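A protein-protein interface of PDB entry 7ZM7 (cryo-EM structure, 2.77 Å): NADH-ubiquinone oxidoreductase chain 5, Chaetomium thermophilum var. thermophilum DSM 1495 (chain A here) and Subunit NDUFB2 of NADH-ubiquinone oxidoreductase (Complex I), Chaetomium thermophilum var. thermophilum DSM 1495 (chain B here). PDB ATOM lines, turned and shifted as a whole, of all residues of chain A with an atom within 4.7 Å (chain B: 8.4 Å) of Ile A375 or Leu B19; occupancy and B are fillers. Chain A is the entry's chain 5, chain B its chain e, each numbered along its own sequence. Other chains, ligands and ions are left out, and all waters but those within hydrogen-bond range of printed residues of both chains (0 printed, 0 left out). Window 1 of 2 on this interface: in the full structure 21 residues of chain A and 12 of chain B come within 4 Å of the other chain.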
ATOM      1  N   LEU A 338      25.227  15.502  -7.722  1.00  0.00           N
ATOM      2  CA  LEU A 338      24.300  16.081  -8.678  1.00  0.00           C
ATOM      3  C   LEU A 338      22.910  16.226  -8.077  1.00  0.00           C
ATOM      4  O   LEU A 338      22.236  17.243  -8.281  1.00  0.00           O
ATOM      5  CB  LEU A 338      24.268  15.216  -9.925  1.00  0.00           C
ATOM      6  CG  LEU A 338      23.492  15.863 -11.050  1.00  0.00           C
ATOM      7  CD1 LEU A 338      24.112  17.196 -11.334  1.00  0.00           C
ATOM      8  CD2 LEU A 338      23.522  14.969 -12.249  1.00  0.00           C
ATOM      9  N   LEU A 368      15.387  22.459 -16.326  1.00  0.00           N
ATOM     10  CA  LEU A 368      16.738  21.847 -16.292  1.00  0.00           C
ATOM     11  C   LEU A 368      16.883  20.982 -15.057  1.00  0.00           C
ATOM     12  O   LEU A 368      17.443  19.896 -15.153  1.00  0.00           O
ATOM     13  CB  LEU A 368      17.823  22.921 -16.383  1.00  0.00           C
ATOM     14  CG  LEU A 368      19.260  22.407 -16.316  1.00  0.00           C
ATOM     15  CD1 LEU A 368      19.773  22.041 -17.693  1.00  0.00           C
ATOM     16  CD2 LEU A 368      20.177  23.429 -15.664  1.00  0.00           C
ATOM     17  N   SER A 371      15.441  17.332 -15.429  1.00  0.00           N
ATOM     18  CA  SER A 371      16.215  16.459 -16.299  1.00  0.00           C
ATOM     19  C   SER A 371      17.500  16.026 -15.626  1.00  0.00           C
ATOM     20  O   SER A 371      17.769  14.830 -15.505  1.00  0.00           O
ATOM     21  CB  SER A 371      16.534  17.169 -17.607  1.00  0.00           C
ATOM     22  OG  SER A 371      17.667  17.995 -17.442  1.00  0.00           O
ATOM     23  N   VAL A 372      18.297  16.993 -15.183  1.00  0.00           N
ATOM     24  CA  VAL A 372      19.606  16.705 -14.528  1.00  0.00           C
ATOM     25  C   VAL A 372      19.381  15.805 -13.317  1.00  0.00           C
ATOM     26  O   VAL A 372      20.192  14.912 -13.110  1.00  0.00           O
ATOM     27  CB  VAL A 372      20.324  18.019 -14.169  1.00  0.00           C
ATOM     28  CG1 VAL A 372      20.935  18.033 -12.780  1.00  0.00           C
ATOM     29  CG2 VAL A 372      21.316  18.458 -15.230  1.00  0.00           C
ATOM     30  N   MET A 373      18.317  16.043 -12.551  1.00  0.00           N
ATOM     31  CA  MET A 373      18.028  15.236 -11.347  1.00  0.00           C
ATOM     32  C   MET A 373      17.557  13.860 -11.782  1.00  0.00           C
ATOM     33  O   MET A 373      17.748  12.903 -11.033  1.00  0.00           O
ATOM     34  CB  MET A 373      16.987  15.900 -10.447  1.00  0.00           C
ATOM     35  CG  MET A 373      17.582  16.928  -9.524  1.00  0.00           C
ATOM     36  SD  MET A 373      16.510  17.220  -8.115  1.00  0.00           S
ATOM     37  CE  MET A 373      16.949  15.831  -7.074  1.00  0.00           C
ATOM     38  N   LEU A 374      16.941  13.783 -12.945  1.00  0.00           N
ATOM     39  CA  LEU A 374      16.592  12.476 -13.469  1.00  0.00           C
ATOM     40  C   LEU A 374      17.767  11.816 -14.167  1.00  0.00           C
ATOM     41  O   LEU A 374      17.806  10.588 -14.247  1.00  0.00           O
ATOM     42  CB  LEU A 374      15.423  12.634 -14.438  1.00  0.00           C
ATOM     43  CG  LEU A 374      14.755  11.451 -15.120  1.00  0.00           C
ATOM     44  CD1 LEU A 374      14.123  10.570 -14.080  1.00  0.00           C
ATOM     45  CD2 LEU A 374      13.740  11.932 -16.139  1.00  0.00           C
ATOM     46  N   ILE A 375      18.715  12.611 -14.679  1.00  0.00           N
ATOM     47  CA  ILE A 375      20.021  12.087 -15.069  1.00  0.00           C
ATOM     48  C   ILE A 375      20.648  11.353 -13.900  1.00  0.00           C
ATOM     49  O   ILE A 375      21.244  10.284 -14.054  1.00  0.00           O
ATOM     50  CB  ILE A 375      20.939  13.224 -15.557  1.00  0.00           C
ATOM     51  CG1 ILE A 375      20.340  14.014 -16.723  1.00  0.00           C
ATOM     52  CG2 ILE A 375      22.322  12.709 -15.894  1.00  0.00           C
ATOM     53  CD1 ILE A 375      20.339  13.294 -18.028  1.00  0.00           C
ATOM     54  N   ALA A 376      20.533  11.938 -12.714  1.00  0.00           N
ATOM     55  CA  ALA A 376      21.144  11.400 -11.516  1.00  0.00           C
ATOM     56  C   ALA A 376      20.394  10.190 -10.987  1.00  0.00           C
ATOM     57  O   ALA A 376      21.022   9.211 -10.574  1.00  0.00           O
ATOM     58  CB  ALA A 376      21.221  12.489 -10.458  1.00  0.00           C
ATOM     59  N   SER A 377      19.072  10.227 -11.033  1.00  0.00           N
ATOM     60  CA  SER A 377      18.275   9.133 -10.432  1.00  0.00           C
ATOM     61  C   SER A 377      18.415   7.892 -11.293  1.00  0.00           C
ATOM     62  O   SER A 377      18.398   6.803 -10.727  1.00  0.00           O
ATOM     63  CB  SER A 377      16.858   9.553 -10.302  1.00  0.00           C
ATOM     64  OG  SER A 377      16.766  10.742  -9.533  1.00  0.00           O
ATOM     65  N   LEU A 378      18.563   8.072 -12.606  1.00  0.00           N
ATOM     66  CA  LEU A 378      18.771   6.933 -13.534  1.00  0.00           C
ATOM     67  C   LEU A 378      20.109   6.259 -13.233  1.00  0.00           C
ATOM     68  O   LEU A 378      20.175   5.047 -13.330  1.00  0.00           O
ATOM     69  CB  LEU A 378      18.616   7.381 -14.987  1.00  0.00           C
ATOM     70  CG  LEU A 378      17.191   7.340 -15.527  1.00  0.00           C
ATOM     71  CD1 LEU A 378      17.198   6.971 -16.998  1.00  0.00           C
ATOM     72  CD2 LEU A 378      16.358   6.339 -14.747  1.00  0.00           C
ATOM     73  N   SER A 379      21.128   7.025 -12.876  1.00  0.00           N
ATOM     74  CA  SER A 379      22.426   6.423 -12.476  1.00  0.00           C
ATOM     75  C   SER A 379      22.398   5.984 -11.005  1.00  0.00           C
ATOM     76  O   SER A 379      23.055   4.991 -10.685  1.00  0.00           O
ATOM     77  CB  SER A 379      23.571   7.343 -12.803  1.00  0.00           C
ATOM     78  OG  SER A 379      23.278   8.669 -12.408  1.00  0.00           O
ATOM     79  N   VAL A 475      24.973  21.038 -15.031  1.00  0.00           N
ATOM     80  CA  VAL A 475      25.099  20.505 -16.380  1.00  0.00           C
ATOM     81  C   VAL A 475      26.411  19.736 -16.540  1.00  0.00           C
ATOM     82  O   VAL A 475      26.464  18.720 -17.240  1.00  0.00           O
ATOM     83  CB  VAL A 475      24.947  21.636 -17.416  1.00  0.00           C
ATOM     84  CG1 VAL A 475      26.003  22.679 -17.234  1.00  0.00           C
ATOM     85  CG2 VAL A 475      25.005  21.081 -18.821  1.00  0.00           C
ATOM     86  N   ALA A 478      26.152  16.452 -14.598  1.00  0.00           N
ATOM     87  CA  ALA A 478      25.296  15.518 -15.317  1.00  0.00           C
ATOM     88  C   ALA A 478      26.028  14.880 -16.490  1.00  0.00           C
ATOM     89  O   ALA A 478      25.808  13.708 -16.806  1.00  0.00           O
ATOM     90  CB  ALA A 478      24.032  16.229 -15.794  1.00  0.00           C
ATOM     91  N   LEU A 479      26.898  15.635 -17.153  1.00  0.00           N
ATOM     92  CA  LEU A 479      27.685  15.048 -18.229  1.00  0.00           C
ATOM     93  C   LEU A 479      28.596  13.954 -17.707  1.00  0.00           C
ATOM     94  O   LEU A 479      28.851  12.971 -18.407  1.00  0.00           O
ATOM     95  CB  LEU A 479      28.489  16.123 -18.956  1.00  0.00           C
ATOM     96  CG  LEU A 479      27.664  16.945 -19.940  1.00  0.00           C
ATOM     97  CD1 LEU A 479      28.534  17.962 -20.658  1.00  0.00           C
ATOM     98  CD2 LEU A 479      26.972  16.027 -20.927  1.00  0.00           C
ATOM     99  N   SER A 481      27.730  12.091 -14.993  1.00  0.00           N
ATOM    100  CA  SER A 481      26.845  11.028 -14.539  1.00  0.00           C
ATOM    101  C   SER A 481      26.405  10.112 -15.662  1.00  0.00           C
ATOM    102  O   SER A 481      25.759   9.098 -15.391  1.00  0.00           O
ATOM    103  CB  SER A 481      25.614  11.624 -13.857  1.00  0.00           C
ATOM    104  OG  SER A 481      25.926  12.101 -12.568  1.00  0.00           O
ATOM    105  N   ILE A 482      26.735  10.446 -16.902  1.00  0.00           N
ATOM    106  CA  ILE A 482      26.352   9.654 -18.060  1.00  0.00           C
ATOM    107  C   ILE A 482      27.525   8.851 -18.599  1.00  0.00           C
ATOM    108  O   ILE A 482      27.456   7.627 -18.699  1.00  0.00           O
ATOM    109  CB  ILE A 482      25.757  10.569 -19.152  1.00  0.00           C
ATOM    110  CG1 ILE A 482      24.523  11.294 -18.628  1.00  0.00           C
ATOM    111  CG2 ILE A 482      25.362   9.751 -20.349  1.00  0.00           C
ATOM    112  CD1 ILE A 482      23.355  10.380 -18.381  1.00  0.00           C
ATOM    113  N   HIS B  12      18.011  27.790 -20.842  1.00  0.00           N
ATOM    114  CA  HIS B  12      17.775  26.746 -19.808  1.00  0.00           C
ATOM    115  C   HIS B  12      17.001  25.574 -20.419  1.00  0.00           C
ATOM    116  O   HIS B  12      17.378  24.419 -20.151  1.00  0.00           O
ATOM    117  CB  HIS B  12      17.047  27.338 -18.595  1.00  0.00           C
ATOM    118  CG  HIS B  12      17.931  28.128 -17.690  1.00  0.00           C
ATOM    119  ND1 HIS B  12      18.259  29.444 -17.943  1.00  0.00           N
ATOM    120  CD2 HIS B  12      18.551  27.796 -16.538  1.00  0.00           C
ATOM    121  CE1 HIS B  12      19.045  29.891 -16.985  1.00  0.00           C
ATOM    122  NE2 HIS B  12      19.239  28.897 -16.111  1.00  0.00           N
ATOM    123  N   ARG B  13      15.961  25.868 -21.205  1.00  0.00           N
ATOM    124  CA  ARG B  13      15.161  24.791 -21.846  1.00  0.00           C
ATOM    125  C   ARG B  13      16.040  24.012 -22.828  1.00  0.00           C
ATOM    126  O   ARG B  13      15.949  22.771 -22.839  1.00  0.00           O
ATOM    127  CB  ARG B  13      13.905  25.348 -22.520  1.00  0.00           C
ATOM    128  CG  ARG B  13      12.891  25.926 -21.546  1.00  0.00           C
ATOM    129  CD  ARG B  13      11.548  26.195 -22.195  1.00  0.00           C
ATOM    130  NE  ARG B  13      11.659  26.953 -23.432  1.00  0.00           N
ATOM    131  CZ  ARG B  13      11.600  28.276 -23.515  1.00  0.00           C
ATOM    132  NH1 ARG B  13      11.708  28.871 -24.690  1.00  0.00           N
ATOM    133  NH2 ARG B  13      11.431  29.001 -22.423  1.00  0.00           N
ATOM    134  N   PHE B  14      16.863  24.711 -23.611  1.00  0.00           N
ATOM    135  CA  PHE B  14      17.684  24.010 -24.628  1.00  0.00           C
ATOM    136  C   PHE B  14      18.645  23.066 -23.912  1.00  0.00           C
ATOM    137  O   PHE B  14      18.770  21.906 -24.336  1.00  0.00           O
ATOM    138  CB  PHE B  14      18.456  25.008 -25.491  1.00  0.00           C
ATOM    139  CG  PHE B  14      19.489  24.385 -26.394  1.00  0.00           C
ATOM    140  CD1 PHE B  14      19.110  23.631 -27.492  1.00  0.00           C
ATOM    141  CD2 PHE B  14      20.841  24.555 -26.147  1.00  0.00           C
ATOM    142  CE1 PHE B  14      20.061  23.057 -28.320  1.00  0.00           C
ATOM    143  CE2 PHE B  14      21.792  23.981 -26.977  1.00  0.00           C
ATOM    144  CZ  PHE B  14      21.400  23.234 -28.062  1.00  0.00           C
ATOM    145  N   LEU B  15      19.273  23.542 -22.835  1.00  0.00           N
ATOM    146  CA  LEU B  15      20.274  22.685 -22.157  1.00  0.00           C
ATOM    147  C   LEU B  15      19.559  21.452 -21.618  1.00  0.00           C
ATOM    148  O   LEU B  15      20.081  20.352 -21.816  1.00  0.00           O
ATOM    149  CB  LEU B  15      20.938  23.462 -21.019  1.00  0.00           C
ATOM    150  CG  LEU B  15      22.233  24.180 -21.386  1.00  0.00           C
ATOM    151  CD1 LEU B  15      22.860  24.817 -20.156  1.00  0.00           C
ATOM    152  CD2 LEU B  15      23.209  23.216 -22.039  1.00  0.00           C
ATOM    153  N   ALA B  16      18.388  21.635 -21.009  1.00  0.00           N
ATOM    154  CA  ALA B  16      17.691  20.487 -20.382  1.00  0.00           C
ATOM    155  C   ALA B  16      17.290  19.446 -21.431  1.00  0.00           C
ATOM    156  O   ALA B  16      17.485  18.252 -21.175  1.00  0.00           O
ATOM    157  CB  ALA B  16      16.494  20.972 -19.607  1.00  0.00           C
ATOM    158  N   THR B  17      16.751  19.892 -22.568  1.00  0.00           N
ATOM    159  CA  THR B  17      16.338  18.946 -23.638  1.00  0.00           C
ATOM    160  C   THR B  17      17.574  18.243 -24.202  1.00  0.00           C
ATOM    161  O   THR B  17      17.500  17.033 -24.455  1.00  0.00           O
ATOM    162  CB  THR B  17      15.502  19.652 -24.710  1.00  0.00           C
ATOM    163  OG1 THR B  17      14.444  20.338 -24.042  1.00  0.00           O
ATOM    164  CG2 THR B  17      14.929  18.698 -25.733  1.00  0.00           C
ATOM    165  N   GLY B  18      18.664  18.985 -24.391  1.00  0.00           N
ATOM    166  CA  GLY B  18      19.896  18.401 -24.951  1.00  0.00           C
ATOM    167  C   GLY B  18      20.468  17.364 -24.013  1.00  0.00           C
ATOM    168  O   GLY B  18      20.914  16.318 -24.494  1.00  0.00           O
ATOM    169  N   LEU B  19      20.507  17.666 -22.719  1.00  0.00           N
ATOM    170  CA  LEU B  19      20.933  16.654 -21.762  1.00  0.00           C
ATOM    171  C   LEU B  19      20.005  15.452 -21.783  1.00  0.00           C
ATOM    172  O   LEU B  19      20.434  14.332 -21.490  1.00  0.00           O
ATOM    173  CB  LEU B  19      21.003  17.258 -20.366  1.00  0.00           C
ATOM    174  CG  LEU B  19      22.127  18.275 -20.229  1.00  0.00           C
ATOM    175  CD1 LEU B  19      21.995  19.050 -18.929  1.00  0.00           C
ATOM    176  CD2 LEU B  19      23.464  17.574 -20.311  1.00  0.00           C
ATOM    177  N   GLY B  20      18.734  15.665 -22.116  1.00  0.00           N
ATOM    178  CA  GLY B  20      17.868  14.538 -22.409  1.00  0.00           C
ATOM    179  C   GLY B  20      18.329  13.774 -23.631  1.00  0.00           C
ATOM    180  O   GLY B  20      18.316  12.541 -23.647  1.00  0.00           O
ATOM    181  N   ALA B  21      18.753  14.493 -24.669  1.00  0.00           N
ATOM    182  CA  ALA B  21      19.320  13.836 -25.837  1.00  0.00           C
ATOM    183  C   ALA B  21      20.637  13.145 -25.519  1.00  0.00           C
ATOM    184  O   ALA B  21      21.070  12.283 -26.289  1.00  0.00           O
ATOM    185  CB  ALA B  21      19.520  14.844 -26.968  1.00  0.00           C
ATOM    186  N   SER B  22      21.292  13.511 -24.416  1.00  0.00           N
ATOM    187  CA  SER B  22      22.484  12.781 -24.001  1.00  0.00           C
ATOM    188  C   SER B  22      22.135  11.345 -23.637  1.00  0.00           C
ATOM    189  O   SER B  22      22.774  10.401 -24.114  1.00  0.00           O
ATOM    190  CB  SER B  22      23.156  13.496 -22.830  1.00  0.00           C
ATOM    191  OG  SER B  22      23.812  14.673 -23.267  1.00  0.00           O
ATOM    192  N   MET B  23      21.108  11.156 -22.812  1.00  0.00           N
ATOM    193  CA  MET B  23      20.518   9.834 -22.687  1.00  0.00           C
ATOM    194  C   MET B  23      19.828   9.453 -23.984  1.00  0.00           C
ATOM    195  O   MET B  23      19.758  10.229 -24.941  1.00  0.00           O
ATOM    196  CB  MET B  23      19.475   9.768 -21.583  1.00  0.00           C
ATOM    197  CG  MET B  23      19.705  10.474 -20.295  1.00  0.00           C
ATOM    198  SD  MET B  23      18.440   9.699 -19.265  1.00  0.00           S
ATOM    199  CE  MET B  23      18.884  10.212 -17.633  1.00  0.00           C
ATOM    200  N   TRP B  24      19.307   8.228 -24.008  1.00  0.00           N
ATOM    201  CA  TRP B  24      18.374   7.789 -25.035  1.00  0.00           C
ATOM    202  C   TRP B  24      19.006   7.868 -26.415  1.00  0.00           C
ATOM    203  O   TRP B  24      18.346   7.646 -27.432  1.00  0.00           O
ATOM    204  CB  TRP B  24      17.097   8.626 -24.988  1.00  0.00           C
ATOM    205  CG  TRP B  24      16.616   8.915 -23.607  1.00  0.00           C
ATOM    206  CD1 TRP B  24      16.388  10.137 -23.073  1.00  0.00           C
ATOM    207  CD2 TRP B  24      16.288   7.965 -22.593  1.00  0.00           C
ATOM    208  NE1 TRP B  24      15.943  10.013 -21.786  1.00  0.00           N
ATOM    209  CE2 TRP B  24      15.871   8.685 -21.470  1.00  0.00           C
ATOM    210  CE3 TRP B  24      16.302   6.571 -22.531  1.00  0.00           C
ATOM    211  CZ2 TRP B  24      15.476   8.064 -20.294  1.00  0.00           C
ATOM    212  CZ3 TRP B  24      15.912   5.959 -21.374  1.00  0.00           C
ATOM    213  CH2 TRP B  24      15.505   6.700 -20.266  1.00  0.00           C
ATOM    214  N   PHE B  25      20.231   8.247 -26.459  1.00  0.00           N
ATOM    215  CA  PHE B  25      21.048   8.062 -27.637  1.00  0.00           C
ATOM    216  C   PHE B  25      22.328   7.360 -27.264  1.00  0.00           C
ATOM    217  O   PHE B  25      22.859   6.590 -28.064  1.00  0.00           O
ATOM    218  CB  PHE B  25      21.361   9.385 -28.324  1.00  0.00           C
ATOM    219  CG  PHE B  25      22.047   9.222 -29.641  1.00  0.00           C
ATOM    220  CD1 PHE B  25      21.315   8.995 -30.790  1.00  0.00           C
ATOM    221  CD2 PHE B  25      23.422   9.282 -29.732  1.00  0.00           C
ATOM    222  CE1 PHE B  25      21.942   8.838 -32.003  1.00  0.00           C
ATOM    223  CE2 PHE B  25      24.054   9.128 -30.943  1.00  0.00           C
ATOM    224  CZ  PHE B  25      23.314   8.905 -32.080  1.00  0.00           C
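The indole nitrogen (NE1) of Trp B24 lies close to the side-chain sulfur (SD) of Met B23 (3.6 Å). The backbone carbonyl oxygen of Leu A368 is in hydrogen-bond range of the side-chain hydroxyl of Ser A371, 3.0 Å away. The backbone carbonyl oxygen (O) of Ile A375 lies within hydrogen-bond range of the side-chain hydroxyl (OG) of Ser A379 (3.1 Å).
Of the printed residues of chain B, Ser A371 touches Ala B16 (3.7 Å). Ala A376 touches none of the printed residues of chain B. Printed residues of chain B within 4 Å of Val A475: Leu B19. Ala A478 touches none of the printed residues of chain B. Of chain A, only Leu A368 (3.9 Å), Val A372 (3.8 Å), Ile A375 (3.6 Å), Val A475 (3.6 Å) and Leu A479 (3.9 Å) come within 4 Å of Leu B19. Printed residues of chain A within 4 Å of Met B23: Leu A374 (3.6 Å), Ile A375 (3.4 Å) and Leu A378 (3.7 Å). The nearest residue of chain B that does not touch Ile A375 is Gly B20 (5.0 Å). The nearest printed residue of chain A that does not touch Leu B15 is Val A475 (4.3 Å).
Leu B15 touches Leu A368. CA of Leu A368 touches CB of Ala B16, 3.4 Å away. CD1 of Leu A368 touches CD1 of Leu B19, at 3.9 Å. OG of Ser A371 touches O of Ala B16, at 3.7 Å. Met B23 touches Leu A374. Leu B19 touches Ile A375. Ile A375 touches Met B23 (CA to CE, 3.4 Å). Leu A378 touches Met B23 (CD1 to CE, 3.7 Å). CD1 of Leu A378 touches CH2 of Trp B24, at 3.7 Å. Leu A479 touches Leu B19 (CD2 to CD2, 3.9 Å).
Hydrophobic or aromatic side chains of chain B that line the printed part of chain A: Leu B15, Ala B16, Leu B19, Met B23 and Trp B24. Of the 16 printed residues of chain A, 8 touch a printed residue of chain B. Printed residues of chain A that touch a printed residue of chain B: Leu A368, Ser A371, Val A372, Leu A374, Ile A375, Leu A378, Val A475 and Leu A479. Hydrophobic or aromatic side chains of chain A that line the printed part of chain B: Leu A368, Val A372, Ile A375, Leu A378, Val A475 and Leu A479. Among the printed residues, no Asp or Glu carboxylate lies within 4 Å of a Lys or Arg side-chain nitrogen of the other chain.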
